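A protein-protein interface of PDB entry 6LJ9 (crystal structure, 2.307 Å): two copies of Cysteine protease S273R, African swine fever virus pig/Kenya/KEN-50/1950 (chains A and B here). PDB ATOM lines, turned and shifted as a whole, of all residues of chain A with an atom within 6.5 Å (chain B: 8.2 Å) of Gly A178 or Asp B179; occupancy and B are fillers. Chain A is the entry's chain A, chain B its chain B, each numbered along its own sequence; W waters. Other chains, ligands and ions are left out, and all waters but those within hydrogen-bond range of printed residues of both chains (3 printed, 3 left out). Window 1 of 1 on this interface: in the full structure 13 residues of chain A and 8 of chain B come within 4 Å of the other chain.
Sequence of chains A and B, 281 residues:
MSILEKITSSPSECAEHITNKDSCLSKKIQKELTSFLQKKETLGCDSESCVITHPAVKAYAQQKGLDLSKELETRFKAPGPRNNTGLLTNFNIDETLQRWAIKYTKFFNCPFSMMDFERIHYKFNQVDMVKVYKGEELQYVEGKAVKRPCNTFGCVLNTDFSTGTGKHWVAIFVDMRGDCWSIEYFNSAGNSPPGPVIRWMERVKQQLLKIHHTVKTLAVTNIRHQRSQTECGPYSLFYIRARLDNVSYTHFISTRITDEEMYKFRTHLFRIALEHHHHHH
Of the printed residues of chain B, Asp A175 touches Gly B178 and Asp B179. Of chain B, only Arg B177 (3.1 Å), Gly B178 (3.4 Å) and Asp B179 (3.9 Å) come within 4 Å of Gly A178. Printed residues of chain B within 4 Å of Asp A179: Cys B180 (3.2 Å) and Tyr B249 (2.7 Å). Of the printed residues of chain B, Cys A180 touches Asp B179 (3.4 Å) and Cys B180 (3.4 Å). Of the printed residues of chain B, Ser A182 touches Asp B179 (2.4 Å). Printed residues of chain B within 4 Å of Glu A184: Asp B179 (3.8 Å). His A212 touches none of the printed residues of chain B. Of chain A, only Asp A175 (3.9 Å), Gly A178 (3.9 Å), Cys A180 (3.4 Å), Ser A182 (2.4 Å), Glu A184 (3.8 Å), Arg A243 (3.3 Å) and Tyr A249 (3.2 Å) come within 4 Å of Asp B179. Val B215 touches none of the printed residues of chain A. The nearest residue of chain B that does not touch Gly A178 is Cys B180 (4.2 Å). The nearest residue of chain A that does not touch Asp B179 is Ser A248 (4.7 Å). The nearest printed residue of chain B that does not touch Cys A180 is Gly B178 (5.6 Å).
The guanidinium group (NH2) of Arg A243 is in salt-bridge range of the side-chain carboxylate (OD1) of Asp B179. The backbone NH (N) of Asp A179 sits at hydrogen-bond distance from the backbone carbonyl oxygen (O) of Cys B180 (3.2 Å). The side-chain hydroxyl of Tyr B249 lies within hydrogen-bond range of the side-chain carboxylate of Asp A179 (2.7 Å). The side-chain hydroxyl (OG) of Ser A182 sits close to the side-chain carboxylate (OD2) of Asp B179 (2.4 Å).
Asp A175 touches Gly B178, but with the chains exchanged Gly A178 does not touch Asp B175 (5.6 Å). Asp A179 touches Tyr B249, and with the chains exchanged Tyr A249 touches Asp B179. Ser A182 touches Asp B179, but with the chains exchanged Asp A179 does not touch Ser B182 (5.4 Å). Arg A243 touches Asp B179, but with the chains exchanged Asp A179 does not touch Arg B243 (5.9 Å).
Of the 17 printed residues of chain A, 10 touch a printed residue of chain B. Hydrophobic or aromatic side chains of chain A that line the printed part of chain B: Tyr A249. Among the printed residues, Asp or Glu carboxylates within 4 Å of a Lys or Arg side-chain nitrogen of the other chain: Arg A243 with Asp B179 (3.3 Å).
Water W2 lies within hydrogen-bond range of the backbone NH (N) of Gly A178 (2.7 Å), the backbone NH (N) of Asp B179 (3.2 Å), the backbone carbonyl oxygen (O) of Cys A180 (3.3 Å) and the side-chain carboxylate (OD2) of Asp A175 (3.4 Å). Water W1 lies within hydrogen-bond range of the side-chain amide nitrogen (ND2) of Asn B246 (2.8 Å) and the backbone carbonyl oxygen (O) of Met A176 (3.0 Å). Water W3 lies within hydrogen-bond range of OD2 of Asp B175 (3.1 Å), NH2 of Arg B243 (3.4 Å), OG of Ser B182 (3.4 Å) and OD1 of Asp A179 (3.4 Å).
Asn B246 touches Asn A151 (OD1 to ND2, 3.6 Å). OD2 of Asp A175 touches CA of Gly B178 (3.6 Å). Gly B178 touches Arg A177 (N to CB, 3.97 Å). Gly A178 touches Arg B177 (CA to O, 3.1 Å). Gly A178 touches Gly B178. Asp B179 touches Gly A178. Asp B179 touches Cys A180 (CB to O, 3.4 Å). Glu A184 touches Asp B179. Tyr A249 touches Asp B179. Tyr A249 touches His B213.
The guanidinium group (NE) of Arg B177 lies within salt-bridge range of the side-chain carboxylate (OD1) of Asp B175, 2.6 Å away. The guanidinium group (NH2) of Arg A177 sits at hydrogen-bond distance from the backbone carbonyl oxygen (O) of Arg A243 (2.8 Å). The indole nitrogen (NE1) of Trp A181 sits at hydrogen-bond distance from the backbone carbonyl oxygen (O) of Gly A178 (3.0 Å). A ring nitrogen (NE2) of His A212 is in hydrogen-bond range of the backbone carbonyl oxygen (O) of Asp A179 (2.6 Å). The guanidinium group (NH2) of Arg A243 lies within salt-bridge range of the side-chain carboxylate (OE2) of Glu A184 (2.5 Å).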
ATOM      1  N   ASN A 151      26.400 -11.407  35.424  1.00  0.00           N
ATOM      2  CA  ASN A 151      26.101 -11.433  33.997  1.00  0.00           C
ATOM      3  C   ASN A 151      26.065 -10.037  33.387  1.00  0.00           C
ATOM      4  O   ASN A 151      25.624  -9.879  32.244  1.00  0.00           O
ATOM      5  CB  ASN A 151      24.780 -12.165  33.736  1.00  0.00           C
ATOM      6  CG  ASN A 151      23.626 -11.621  34.563  1.00  0.00           C
ATOM      7  OD1 ASN A 151      23.708 -10.536  35.135  1.00  0.00           O
ATOM      8  ND2 ASN A 151      22.537 -12.381  34.620  1.00  0.00           N
ATOM      9  N   ASP A 175      26.916  -7.000  28.419  1.00  0.00           N
ATOM     10  CA  ASP A 175      25.622  -7.577  28.756  1.00  0.00           C
ATOM     11  C   ASP A 175      25.671  -9.072  28.456  1.00  0.00           C
ATOM     12  O   ASP A 175      25.732  -9.475  27.289  1.00  0.00           O
ATOM     13  CB  ASP A 175      24.503  -6.888  27.978  1.00  0.00           C
ATOM     14  CG  ASP A 175      23.121  -7.287  28.459  1.00  0.00           C
ATOM     15  OD1 ASP A 175      23.019  -8.105  29.397  1.00  0.00           O
ATOM     16  OD2 ASP A 175      22.131  -6.775  27.895  1.00  0.00           O
ATOM     17  N   MET A 176      25.650  -9.885  29.506  1.00  0.00           N
ATOM     18  CA  MET A 176      25.684 -11.336  29.362  1.00  0.00           C
ATOM     19  C   MET A 176      24.392 -11.963  29.880  1.00  0.00           C
ATOM     20  O   MET A 176      24.388 -13.095  30.362  1.00  0.00           O
ATOM     21  CB  MET A 176      26.890 -11.917  30.105  1.00  0.00           C
ATOM     22  CG  MET A 176      28.232 -11.424  29.586  1.00  0.00           C
ATOM     23  SD  MET A 176      29.713 -11.844  30.786  1.00  0.00           S
ATOM     24  CE  MET A 176      29.314 -10.576  32.211  1.00  0.00           C
ATOM     25  N   ARG A 177      23.295 -11.211  29.775  1.00  0.00           N
ATOM     26  CA  ARG A 177      21.989 -11.676  30.226  1.00  0.00           C
ATOM     27  C   ARG A 177      21.180 -12.327  29.112  1.00  0.00           C
ATOM     28  O   ARG A 177      20.451 -13.291  29.362  1.00  0.00           O
ATOM     29  CB  ARG A 177      21.188 -10.510  30.818  1.00  0.00           C
ATOM     30  CG  ARG A 177      21.781  -9.906  32.080  1.00  0.00           C
ATOM     31  CD  ARG A 177      21.106  -8.587  32.420  1.00  0.00           C
ATOM     32  NE  ARG A 177      21.295  -7.599  31.361  1.00  0.00           N
ATOM     33  CZ  ARG A 177      20.923  -6.328  31.450  1.00  0.00           C
ATOM     34  NH1 ARG A 177      20.340  -5.883  32.554  1.00  0.00           N
ATOM     35  NH2 ARG A 177      21.134  -5.498  30.436  1.00  0.00           N
ATOM     36  N   GLY A 178      21.284 -11.823  27.884  1.00  0.00           N
ATOM     37  CA  GLY A 178      20.440 -12.273  26.801  1.00  0.00           C
ATOM     38  C   GLY A 178      21.049 -13.406  25.998  1.00  0.00           C
ATOM     39  O   GLY A 178      22.129 -13.921  26.296  1.00  0.00           O
ATOM     40  N   ASP A 179      20.327 -13.791  24.944  1.00  0.00           N
ATOM     41  CA  ASP A 179      20.794 -14.876  24.094  1.00  0.00           C
ATOM     42  C   ASP A 179      21.956 -14.444  23.214  1.00  0.00           C
ATOM     43  O   ASP A 179      22.734 -15.299  22.774  1.00  0.00           O
ATOM     44  CB  ASP A 179      19.649 -15.413  23.232  1.00  0.00           C
ATOM     45  CG  ASP A 179      19.930 -16.809  22.689  1.00  0.00           C
ATOM     46  OD1 ASP A 179      20.362 -17.681  23.471  1.00  0.00           O
ATOM     47  OD2 ASP A 179      19.712 -17.036  21.480  1.00  0.00           O
ATOM     48  N   CYS A 180      22.093 -13.145  22.958  1.00  0.00           N
ATOM     49  CA  CYS A 180      23.234 -12.577  22.248  1.00  0.00           C
ATOM     50  C   CYS A 180      23.941 -11.618  23.196  1.00  0.00           C
ATOM     51  O   CYS A 180      23.422 -10.536  23.492  1.00  0.00           O
ATOM     52  CB  CYS A 180      22.796 -11.858  20.976  1.00  0.00           C
ATOM     53  SG  CYS A 180      24.023 -10.709  20.323  1.00  0.00           S
ATOM     54  N   TRP A 181      25.113 -12.019  23.676  1.00  0.00           N
ATOM     55  CA  TRP A 181      25.901 -11.165  24.547  1.00  0.00           C
ATOM     56  C   TRP A 181      26.566 -10.064  23.732  1.00  0.00           C
ATOM     57  O   TRP A 181      26.956 -10.263  22.579  1.00  0.00           O
ATOM     58  CB  TRP A 181      26.957 -11.983  25.293  1.00  0.00           C
ATOM     59  CG  TRP A 181      26.374 -13.039  26.191  1.00  0.00           C
ATOM     60  CD1 TRP A 181      25.052 -13.319  26.376  1.00  0.00           C
ATOM     61  CD2 TRP A 181      27.097 -13.951  27.029  1.00  0.00           C
ATOM     62  NE1 TRP A 181      24.906 -14.349  27.272  1.00  0.00           N
ATOM     63  CE2 TRP A 181      26.146 -14.755  27.689  1.00  0.00           C
ATOM     64  CE3 TRP A 181      28.454 -14.167  27.284  1.00  0.00           C
ATOM     65  CZ2 TRP A 181      26.508 -15.756  28.588  1.00  0.00           C
ATOM     66  CZ3 TRP A 181      28.813 -15.162  28.178  1.00  0.00           C
ATOM     67  CH2 TRP A 181      27.843 -15.944  28.818  1.00  0.00           C
ATOM     68  N   SER A 182      26.684  -8.888  24.340  1.00  0.00           N
ATOM     69  CA  SER A 182      27.204  -7.720  23.649  1.00  0.00           C
ATOM     70  C   SER A 182      28.243  -7.018  24.508  1.00  0.00           C
ATOM     71  O   SER A 182      28.067  -6.872  25.722  1.00  0.00           O
ATOM     72  CB  SER A 182      26.081  -6.742  23.286  1.00  0.00           C
ATOM     73  OG  SER A 182      25.363  -6.340  24.440  1.00  0.00           O
ATOM     74  N   ILE A 183      29.326  -6.594  23.867  1.00  0.00           N
ATOM     75  CA  ILE A 183      30.341  -5.742  24.473  1.00  0.00           C
ATOM     76  C   ILE A 183      30.150  -4.351  23.888  1.00  0.00           C
ATOM     77  O   ILE A 183      30.291  -4.157  22.674  1.00  0.00           O
ATOM     78  CB  ILE A 183      31.757  -6.276  24.212  1.00  0.00           C
ATOM     79  CG1 ILE A 183      31.874  -7.718  24.713  1.00  0.00           C
ATOM     80  CG2 ILE A 183      32.792  -5.393  24.884  1.00  0.00           C
ATOM     81  CD1 ILE A 183      33.051  -8.468  24.136  1.00  0.00           C
ATOM     82  N   GLU A 184      29.813  -3.388  24.740  1.00  0.00           N
ATOM     83  CA  GLU A 184      29.325  -2.091  24.294  1.00  0.00           C
ATOM     84  C   GLU A 184      30.278  -0.982  24.716  1.00  0.00           C
ATOM     85  O   GLU A 184      30.774  -0.969  25.846  1.00  0.00           O
ATOM     86  CB  GLU A 184      27.925  -1.825  24.854  1.00  0.00           C
ATOM     87  CG  GLU A 184      26.954  -2.973  24.624  1.00  0.00           C
ATOM     88  CD  GLU A 184      25.695  -2.850  25.458  1.00  0.00           C
ATOM     89  OE1 GLU A 184      25.453  -1.760  26.016  1.00  0.00           O
ATOM     90  OE2 GLU A 184      24.949  -3.847  25.560  1.00  0.00           O
ATOM     91  N   HIS A 212      29.799 -19.013  25.440  1.00  0.00           N
ATOM     92  CA  HIS A 212      28.564 -18.634  24.769  1.00  0.00           C
ATOM     93  C   HIS A 212      28.800 -18.617  23.267  1.00  0.00           C
ATOM     94  O   HIS A 212      29.936 -18.510  22.797  1.00  0.00           O
ATOM     95  CB  HIS A 212      28.047 -17.270  25.246  1.00  0.00           C
ATOM     96  CG  HIS A 212      26.619 -17.003  24.878  1.00  0.00           C
ATOM     97  ND1 HIS A 212      25.585 -17.827  25.265  1.00  0.00           N
ATOM     98  CD2 HIS A 212      26.054 -16.003  24.160  1.00  0.00           C
ATOM     99  CE1 HIS A 212      24.444 -17.347  24.802  1.00  0.00           C
ATOM    100  NE2 HIS A 212      24.702 -16.240  24.129  1.00  0.00           N
ATOM    101  N   THR A 214      26.992 -16.556  20.875  1.00  0.00           N
ATOM    102  CA  THR A 214      26.742 -15.295  20.181  1.00  0.00           C
ATOM    103  C   THR A 214      27.272 -14.149  21.031  1.00  0.00           C
ATOM    104  O   THR A 214      26.688 -13.820  22.069  1.00  0.00           O
ATOM    105  CB  THR A 214      25.253 -15.110  19.892  1.00  0.00           C
ATOM    106  OG1 THR A 214      24.732 -16.301  19.291  1.00  0.00           O
ATOM    107  CG2 THR A 214      25.041 -13.939  18.946  1.00  0.00           C
ATOM    108  N   ARG A 243      21.217   0.526  30.881  1.00  0.00           N
ATOM    109  CA  ARG A 243      21.389  -0.858  30.449  1.00  0.00           C
ATOM    110  C   ARG A 243      21.093  -1.827  31.587  1.00  0.00           C
ATOM    111  O   ARG A 243      20.566  -2.923  31.359  1.00  0.00           O
ATOM    112  CB  ARG A 243      22.805  -1.078  29.917  1.00  0.00           C
ATOM    113  CG  ARG A 243      23.175  -0.213  28.722  1.00  0.00           C
ATOM    114  CD  ARG A 243      22.494  -0.672  27.444  1.00  0.00           C
ATOM    115  NE  ARG A 243      22.968  -1.981  27.006  1.00  0.00           N
ATOM    116  CZ  ARG A 243      22.270  -3.106  27.122  1.00  0.00           C
ATOM    117  NH1 ARG A 243      21.058  -3.082  27.657  1.00  0.00           N
ATOM    118  NH2 ARG A 243      22.780  -4.253  26.697  1.00  0.00           N
ATOM    119  N   VAL A 247      17.246  -0.929  29.413  1.00  0.00           N
ATOM    120  CA  VAL A 247      17.054  -0.058  28.258  1.00  0.00           C
ATOM    121  C   VAL A 247      18.030  -0.509  27.178  1.00  0.00           C
ATOM    122  O   VAL A 247      19.247  -0.521  27.395  1.00  0.00           O
ATOM    123  CB  VAL A 247      17.269   1.418  28.622  1.00  0.00           C
ATOM    124  CG1 VAL A 247      17.193   2.292  27.374  1.00  0.00           C
ATOM    125  CG2 VAL A 247      16.241   1.866  29.651  1.00  0.00           C
ATOM    126  N   SER A 248      17.500  -0.895  26.020  1.00  0.00           N
ATOM    127  CA  SER A 248      18.339  -1.432  24.957  1.00  0.00           C
ATOM    128  C   SER A 248      19.329  -0.384  24.462  1.00  0.00           C
ATOM    129  O   SER A 248      19.070   0.822  24.509  1.00  0.00           O
ATOM    130  CB  SER A 248      17.475  -1.926  23.794  1.00  0.00           C
ATOM    131  OG  SER A 248      18.279  -2.422  22.736  1.00  0.00           O
ATOM    132  N   TYR A 249      20.486  -0.859  23.990  1.00  0.00           N
ATOM    133  CA  TYR A 249      21.484   0.042  23.424  1.00  0.00           C
ATOM    134  C   TYR A 249      20.986   0.722  22.156  1.00  0.00           C
ATOM    135  O   TYR A 249      21.501   1.786  21.793  1.00  0.00           O
ATOM    136  CB  TYR A 249      22.786  -0.715  23.137  1.00  0.00           C
ATOM    137  CG  TYR A 249      22.634  -1.922  22.229  1.00  0.00           C
ATOM    138  CD1 TYR A 249      22.398  -1.772  20.866  1.00  0.00           C
ATOM    139  CD2 TYR A 249      22.747  -3.209  22.732  1.00  0.00           C
ATOM    140  CE1 TYR A 249      22.266  -2.867  20.037  1.00  0.00           C
ATOM    141  CE2 TYR A 249      22.617  -4.311  21.908  1.00  0.00           C
ATOM    142  CZ  TYR A 249      22.377  -4.134  20.563  1.00  0.00           C
ATOM    143  OH  TYR A 249      22.247  -5.232  19.743  1.00  0.00           O
ATOM    144  N   ASP B 175      12.082 -15.728  27.438  1.00  0.00           N
ATOM    145  CA  ASP B 175      13.258 -15.052  27.976  1.00  0.00           C
ATOM    146  C   ASP B 175      13.354 -13.674  27.332  1.00  0.00           C
ATOM    147  O   ASP B 175      13.678 -13.559  26.146  1.00  0.00           O
ATOM    148  CB  ASP B 175      14.520 -15.873  27.722  1.00  0.00           C
ATOM    149  CG  ASP B 175      15.695 -15.419  28.570  1.00  0.00           C
ATOM    150  OD1 ASP B 175      15.572 -14.384  29.258  1.00  0.00           O
ATOM    151  OD2 ASP B 175      16.740 -16.103  28.552  1.00  0.00           O
ATOM    152  N   MET B 176      13.074 -12.636  28.114  1.00  0.00           N
ATOM    153  CA  MET B 176      13.123 -11.266  27.619  1.00  0.00           C
ATOM    154  C   MET B 176      14.247 -10.482  28.290  1.00  0.00           C
ATOM    155  O   MET B 176      14.205  -9.256  28.371  1.00  0.00           O
ATOM    156  CB  MET B 176      11.778 -10.573  27.844  1.00  0.00           C
ATOM    157  CG  MET B 176      10.653 -11.140  26.994  1.00  0.00           C
ATOM    158  SD  MET B 176       8.887 -10.629  27.634  1.00  0.00           S
ATOM    159  CE  MET B 176       8.853 -11.683  29.273  1.00  0.00           C
ATOM    160  N   ARG B 177      15.252 -11.206  28.770  1.00  0.00           N
ATOM    161  CA  ARG B 177      16.438 -10.605  29.359  1.00  0.00           C
ATOM    162  C   ARG B 177      17.485 -10.359  28.281  1.00  0.00           C
ATOM    163  O   ARG B 177      17.591 -11.114  27.310  1.00  0.00           O
ATOM    164  CB  ARG B 177      17.016 -11.513  30.447  1.00  0.00           C
ATOM    165  CG  ARG B 177      16.035 -11.877  31.550  1.00  0.00           C
ATOM    166  CD  ARG B 177      16.548 -13.035  32.398  1.00  0.00           C
ATOM    167  NE  ARG B 177      16.620 -14.284  31.642  1.00  0.00           N
ATOM    168  CZ  ARG B 177      16.871 -15.472  32.183  1.00  0.00           C
ATOM    169  NH1 ARG B 177      17.070 -15.579  33.489  1.00  0.00           N
ATOM    170  NH2 ARG B 177      16.919 -16.555  31.419  1.00  0.00           N
ATOM    171  N   GLY B 178      18.249  -9.283  28.454  1.00  0.00           N
ATOM    172  CA  GLY B 178      19.370  -8.994  27.580  1.00  0.00           C
ATOM    173  C   GLY B 178      19.023  -8.419  26.221  1.00  0.00           C
ATOM    174  O   GLY B 178      18.092  -7.619  26.092  1.00  0.00           O
ATOM    175  N   ASP B 179      19.766  -8.835  25.195  1.00  0.00           N
ATOM    176  CA  ASP B 179      19.714  -8.206  23.881  1.00  0.00           C
ATOM    177  C   ASP B 179      18.909  -8.981  22.851  1.00  0.00           C
ATOM    178  O   ASP B 179      18.388  -8.371  21.911  1.00  0.00           O
ATOM    179  CB  ASP B 179      21.132  -7.998  23.340  1.00  0.00           C
ATOM    180  CG  ASP B 179      21.805  -6.779  23.927  1.00  0.00           C
ATOM    181  OD1 ASP B 179      21.087  -5.832  24.305  1.00  0.00           O
ATOM    182  OD2 ASP B 179      23.048  -6.766  24.010  1.00  0.00           O
ATOM    183  N   CYS B 180      18.796 -10.300  22.983  1.00  0.00           N
ATOM    184  CA  CYS B 180      18.035 -11.111  22.039  1.00  0.00           C
ATOM    185  C   CYS B 180      17.122 -12.046  22.813  1.00  0.00           C
ATOM    186  O   CYS B 180      17.588 -12.816  23.658  1.00  0.00           O
ATOM    187  CB  CYS B 180      18.958 -11.903  21.110  1.00  0.00           C
ATOM    188  SG  CYS B 180      19.726 -10.897  19.820  1.00  0.00           S
ATOM    189  N   TRP B 181      15.829 -11.986  22.513  1.00  0.00           N
ATOM    190  CA  TRP B 181      14.803 -12.681  23.274  1.00  0.00           C
ATOM    191  C   TRP B 181      14.415 -13.989  22.597  1.00  0.00           C
ATOM    192  O   TRP B 181      14.634 -14.187  21.399  1.00  0.00           O
ATOM    193  CB  TRP B 181      13.574 -11.784  23.451  1.00  0.00           C
ATOM    194  CG  TRP B 181      13.871 -10.512  24.195  1.00  0.00           C
ATOM    195  CD1 TRP B 181      15.061 -10.153  24.762  1.00  0.00           C
ATOM    196  CD2 TRP B 181      12.964  -9.434  24.453  1.00  0.00           C
ATOM    197  NE1 TRP B 181      14.950  -8.920  25.356  1.00  0.00           N
ATOM    198  CE2 TRP B 181      13.673  -8.456  25.181  1.00  0.00           C
ATOM    199  CE3 TRP B 181      11.622  -9.199  24.140  1.00  0.00           C
ATOM    200  CZ2 TRP B 181      13.086  -7.265  25.599  1.00  0.00           C
ATOM    201  CZ3 TRP B 181      11.040  -8.014  24.557  1.00  0.00           C
ATOM    202  CH2 TRP B 181      11.772  -7.063  25.279  1.00  0.00           C
ATOM    203  N   SER B 182      13.830 -14.889  23.386  1.00  0.00           N
ATOM    204  CA  SER B 182      13.503 -16.226  22.916  1.00  0.00           C
ATOM    205  C   SER B 182      12.182 -16.686  23.511  1.00  0.00           C
ATOM    206  O   SER B 182      11.873 -16.387  24.668  1.00  0.00           O
ATOM    207  CB  SER B 182      14.609 -17.225  23.273  1.00  0.00           C
ATOM    208  OG  SER B 182      14.829 -17.257  24.672  1.00  0.00           O
ATOM    209  N   HIS B 212      11.278  -4.981  20.812  1.00  0.00           N
ATOM    210  CA  HIS B 212      12.636  -5.498  20.732  1.00  0.00           C
ATOM    211  C   HIS B 212      12.964  -5.843  19.288  1.00  0.00           C
ATOM    212  O   HIS B 212      12.077  -6.153  18.489  1.00  0.00           O
ATOM    213  CB  HIS B 212      12.829  -6.728  21.622  1.00  0.00           C
ATOM    214  CG  HIS B 212      14.249  -6.955  22.031  1.00  0.00           C
ATOM    215  ND1 HIS B 212      14.958  -6.045  22.785  1.00  0.00           N
ATOM    216  CD2 HIS B 212      15.096  -7.982  21.788  1.00  0.00           C
ATOM    217  CE1 HIS B 212      16.179  -6.504  22.993  1.00  0.00           C
ATOM    218  NE2 HIS B 212      16.287  -7.678  22.397  1.00  0.00           N
ATOM    219  N   HIS B 213      14.258  -5.804  18.970  1.00  0.00           N
ATOM    220  CA  HIS B 213      14.692  -5.955  17.587  1.00  0.00           C
ATOM    221  C   HIS B 213      14.769  -7.420  17.168  1.00  0.00           C
ATOM    222  O   HIS B 213      14.385  -7.765  16.045  1.00  0.00           O
ATOM    223  CB  HIS B 213      16.042  -5.265  17.387  1.00  0.00           C
ATOM    224  CG  HIS B 213      17.110  -5.736  18.327  1.00  0.00           C
ATOM    225  ND1 HIS B 213      17.945  -6.791  18.034  1.00  0.00           N
ATOM    226  CD2 HIS B 213      17.480  -5.291  19.551  1.00  0.00           C
ATOM    227  CE1 HIS B 213      18.784  -6.979  19.038  1.00  0.00           C
ATOM    228  NE2 HIS B 213      18.522  -6.082  19.971  1.00  0.00           N
ATOM    229  N   THR B 214      15.255  -8.293  18.047  1.00  0.00           N
ATOM    230  CA  THR B 214      15.440  -9.704  17.729  1.00  0.00           C
ATOM    231  C   THR B 214      14.651 -10.553  18.715  1.00  0.00           C
ATOM    232  O   THR B 214      14.896 -10.496  19.924  1.00  0.00           O
ATOM    233  CB  THR B 214      16.918 -10.088  17.762  1.00  0.00           C
ATOM    234  OG1 THR B 214      17.637  -9.319  16.789  1.00  0.00           O
ATOM    235  CG2 THR B 214      17.086 -11.568  17.454  1.00  0.00           C
ATOM    236  N   VAL B 215      13.708 -11.334  18.194  1.00  0.00           N
ATOM    237  CA  VAL B 215      12.938 -12.290  18.980  1.00  0.00           C
ATOM    238  C   VAL B 215      12.964 -13.620  18.242  1.00  0.00           C
ATOM    239  O   VAL B 215      12.577 -13.690  17.068  1.00  0.00           O
ATOM    240  CB  VAL B 215      11.489 -11.827  19.209  1.00  0.00           C
ATOM    241  CG1 VAL B 215      10.706 -12.900  19.947  1.00  0.00           C
ATOM    242  CG2 VAL B 215      11.465 -10.519  19.986  1.00  0.00           C
ATOM    243  N   LYS B 216      13.421 -14.666  18.920  1.00  0.00           N
ATOM    244  CA  LYS B 216      13.541 -15.992  18.334  1.00  0.00           C
ATOM    245  C   LYS B 216      12.512 -16.928  18.952  1.00  0.00           C
ATOM    246  O   LYS B 216      12.252 -16.873  20.157  1.00  0.00           O
ATOM    247  CB  LYS B 216      14.951 -16.555  18.541  1.00  0.00           C
ATOM    248  CG  LYS B 216      16.057 -15.576  18.185  1.00  0.00           C
ATOM    249  CD  LYS B 216      17.421 -16.246  18.187  1.00  0.00           C
ATOM    250  CE  LYS B 216      18.512 -15.254  17.822  1.00  0.00           C
ATOM    251  NZ  LYS B 216      19.828 -15.919  17.616  1.00  0.00           N
ATOM    252  N   ARG B 243      16.337 -22.320  33.319  1.00  0.00           N
ATOM    253  CA  ARG B 243      16.368 -21.092  32.530  1.00  0.00           C
ATOM    254  C   ARG B 243      16.347 -19.856  33.421  1.00  0.00           C
ATOM    255  O   ARG B 243      16.956 -18.836  33.077  1.00  0.00           O
ATOM    256  CB  ARG B 243      15.194 -21.059  31.552  1.00  0.00           C
ATOM    257  CG  ARG B 243      15.206 -22.169  30.509  1.00  0.00           C
ATOM    258  CD  ARG B 243      16.335 -22.002  29.504  1.00  0.00           C
ATOM    259  NE  ARG B 243      16.182 -20.799  28.690  1.00  0.00           N
ATOM    260  CZ  ARG B 243      16.950 -19.720  28.799  1.00  0.00           C
ATOM    261  NH1 ARG B 243      17.934 -19.690  29.685  1.00  0.00           N
ATOM    262  NH2 ARG B 243      16.737 -18.671  28.015  1.00  0.00           N
ATOM    263  N   ASN B 246      19.759 -18.990  34.503  1.00  0.00           N
ATOM    264  CA  ASN B 246      20.640 -18.617  33.394  1.00  0.00           C
ATOM    265  C   ASN B 246      21.421 -19.802  32.830  1.00  0.00           C
ATOM    266  O   ASN B 246      22.567 -19.647  32.400  1.00  0.00           O
ATOM    267  CB  ASN B 246      21.599 -17.492  33.795  1.00  0.00           C
ATOM    268  CG  ASN B 246      20.910 -16.143  33.886  1.00  0.00           C
ATOM    269  OD1 ASN B 246      20.789 -15.566  34.966  1.00  0.00           O
ATOM    270  ND2 ASN B 246      20.456 -15.633  32.747  1.00  0.00           N
ATOM    271  N   SER B 248      21.594 -21.893  29.628  1.00  0.00           N
ATOM    272  CA  SER B 248      21.117 -21.698  28.268  1.00  0.00           C
ATOM    273  C   SER B 248      20.300 -22.901  27.808  1.00  0.00           C
ATOM    274  O   SER B 248      20.519 -24.035  28.241  1.00  0.00           O
ATOM    275  CB  SER B 248      22.295 -21.463  27.321  1.00  0.00           C
ATOM    276  OG  SER B 248      21.850 -21.234  25.995  1.00  0.00           O
ATOM    277  N   TYR B 249      19.333 -22.635  26.926  1.00  0.00           N
ATOM    278  CA  TYR B 249      18.523 -23.708  26.364  1.00  0.00           C
ATOM    279  C   TYR B 249      19.359 -24.703  25.572  1.00  0.00           C
ATOM    280  O   TYR B 249      18.921 -25.840  25.366  1.00  0.00           O
ATOM    281  CB  TYR B 249      17.424 -23.124  25.474  1.00  0.00           C
ATOM    282  CG  TYR B 249      17.935 -22.216  24.373  1.00  0.00           C
ATOM    283  CD1 TYR B 249      18.483 -22.740  23.207  1.00  0.00           C
ATOM    284  CD2 TYR B 249      17.861 -20.836  24.496  1.00  0.00           C
ATOM    285  CE1 TYR B 249      18.944 -21.916  22.198  1.00  0.00           C
ATOM    286  CE2 TYR B 249      18.322 -20.004  23.492  1.00  0.00           C
ATOM    287  CZ  TYR B 249      18.862 -20.549  22.346  1.00  0.00           C
ATOM    288  OH  TYR B 249      19.323 -19.726  21.344  1.00  0.00           O
HETATM  289  O   HOH W   1      22.964 -15.475  31.622  1.00  0.00           O
HETATM  290  O   HOH W   2      22.433  -9.853  26.527  1.00  0.00           O
HETATM  291  O   HOH W   3      18.015 -16.514  25.711  1.00  0.00           O
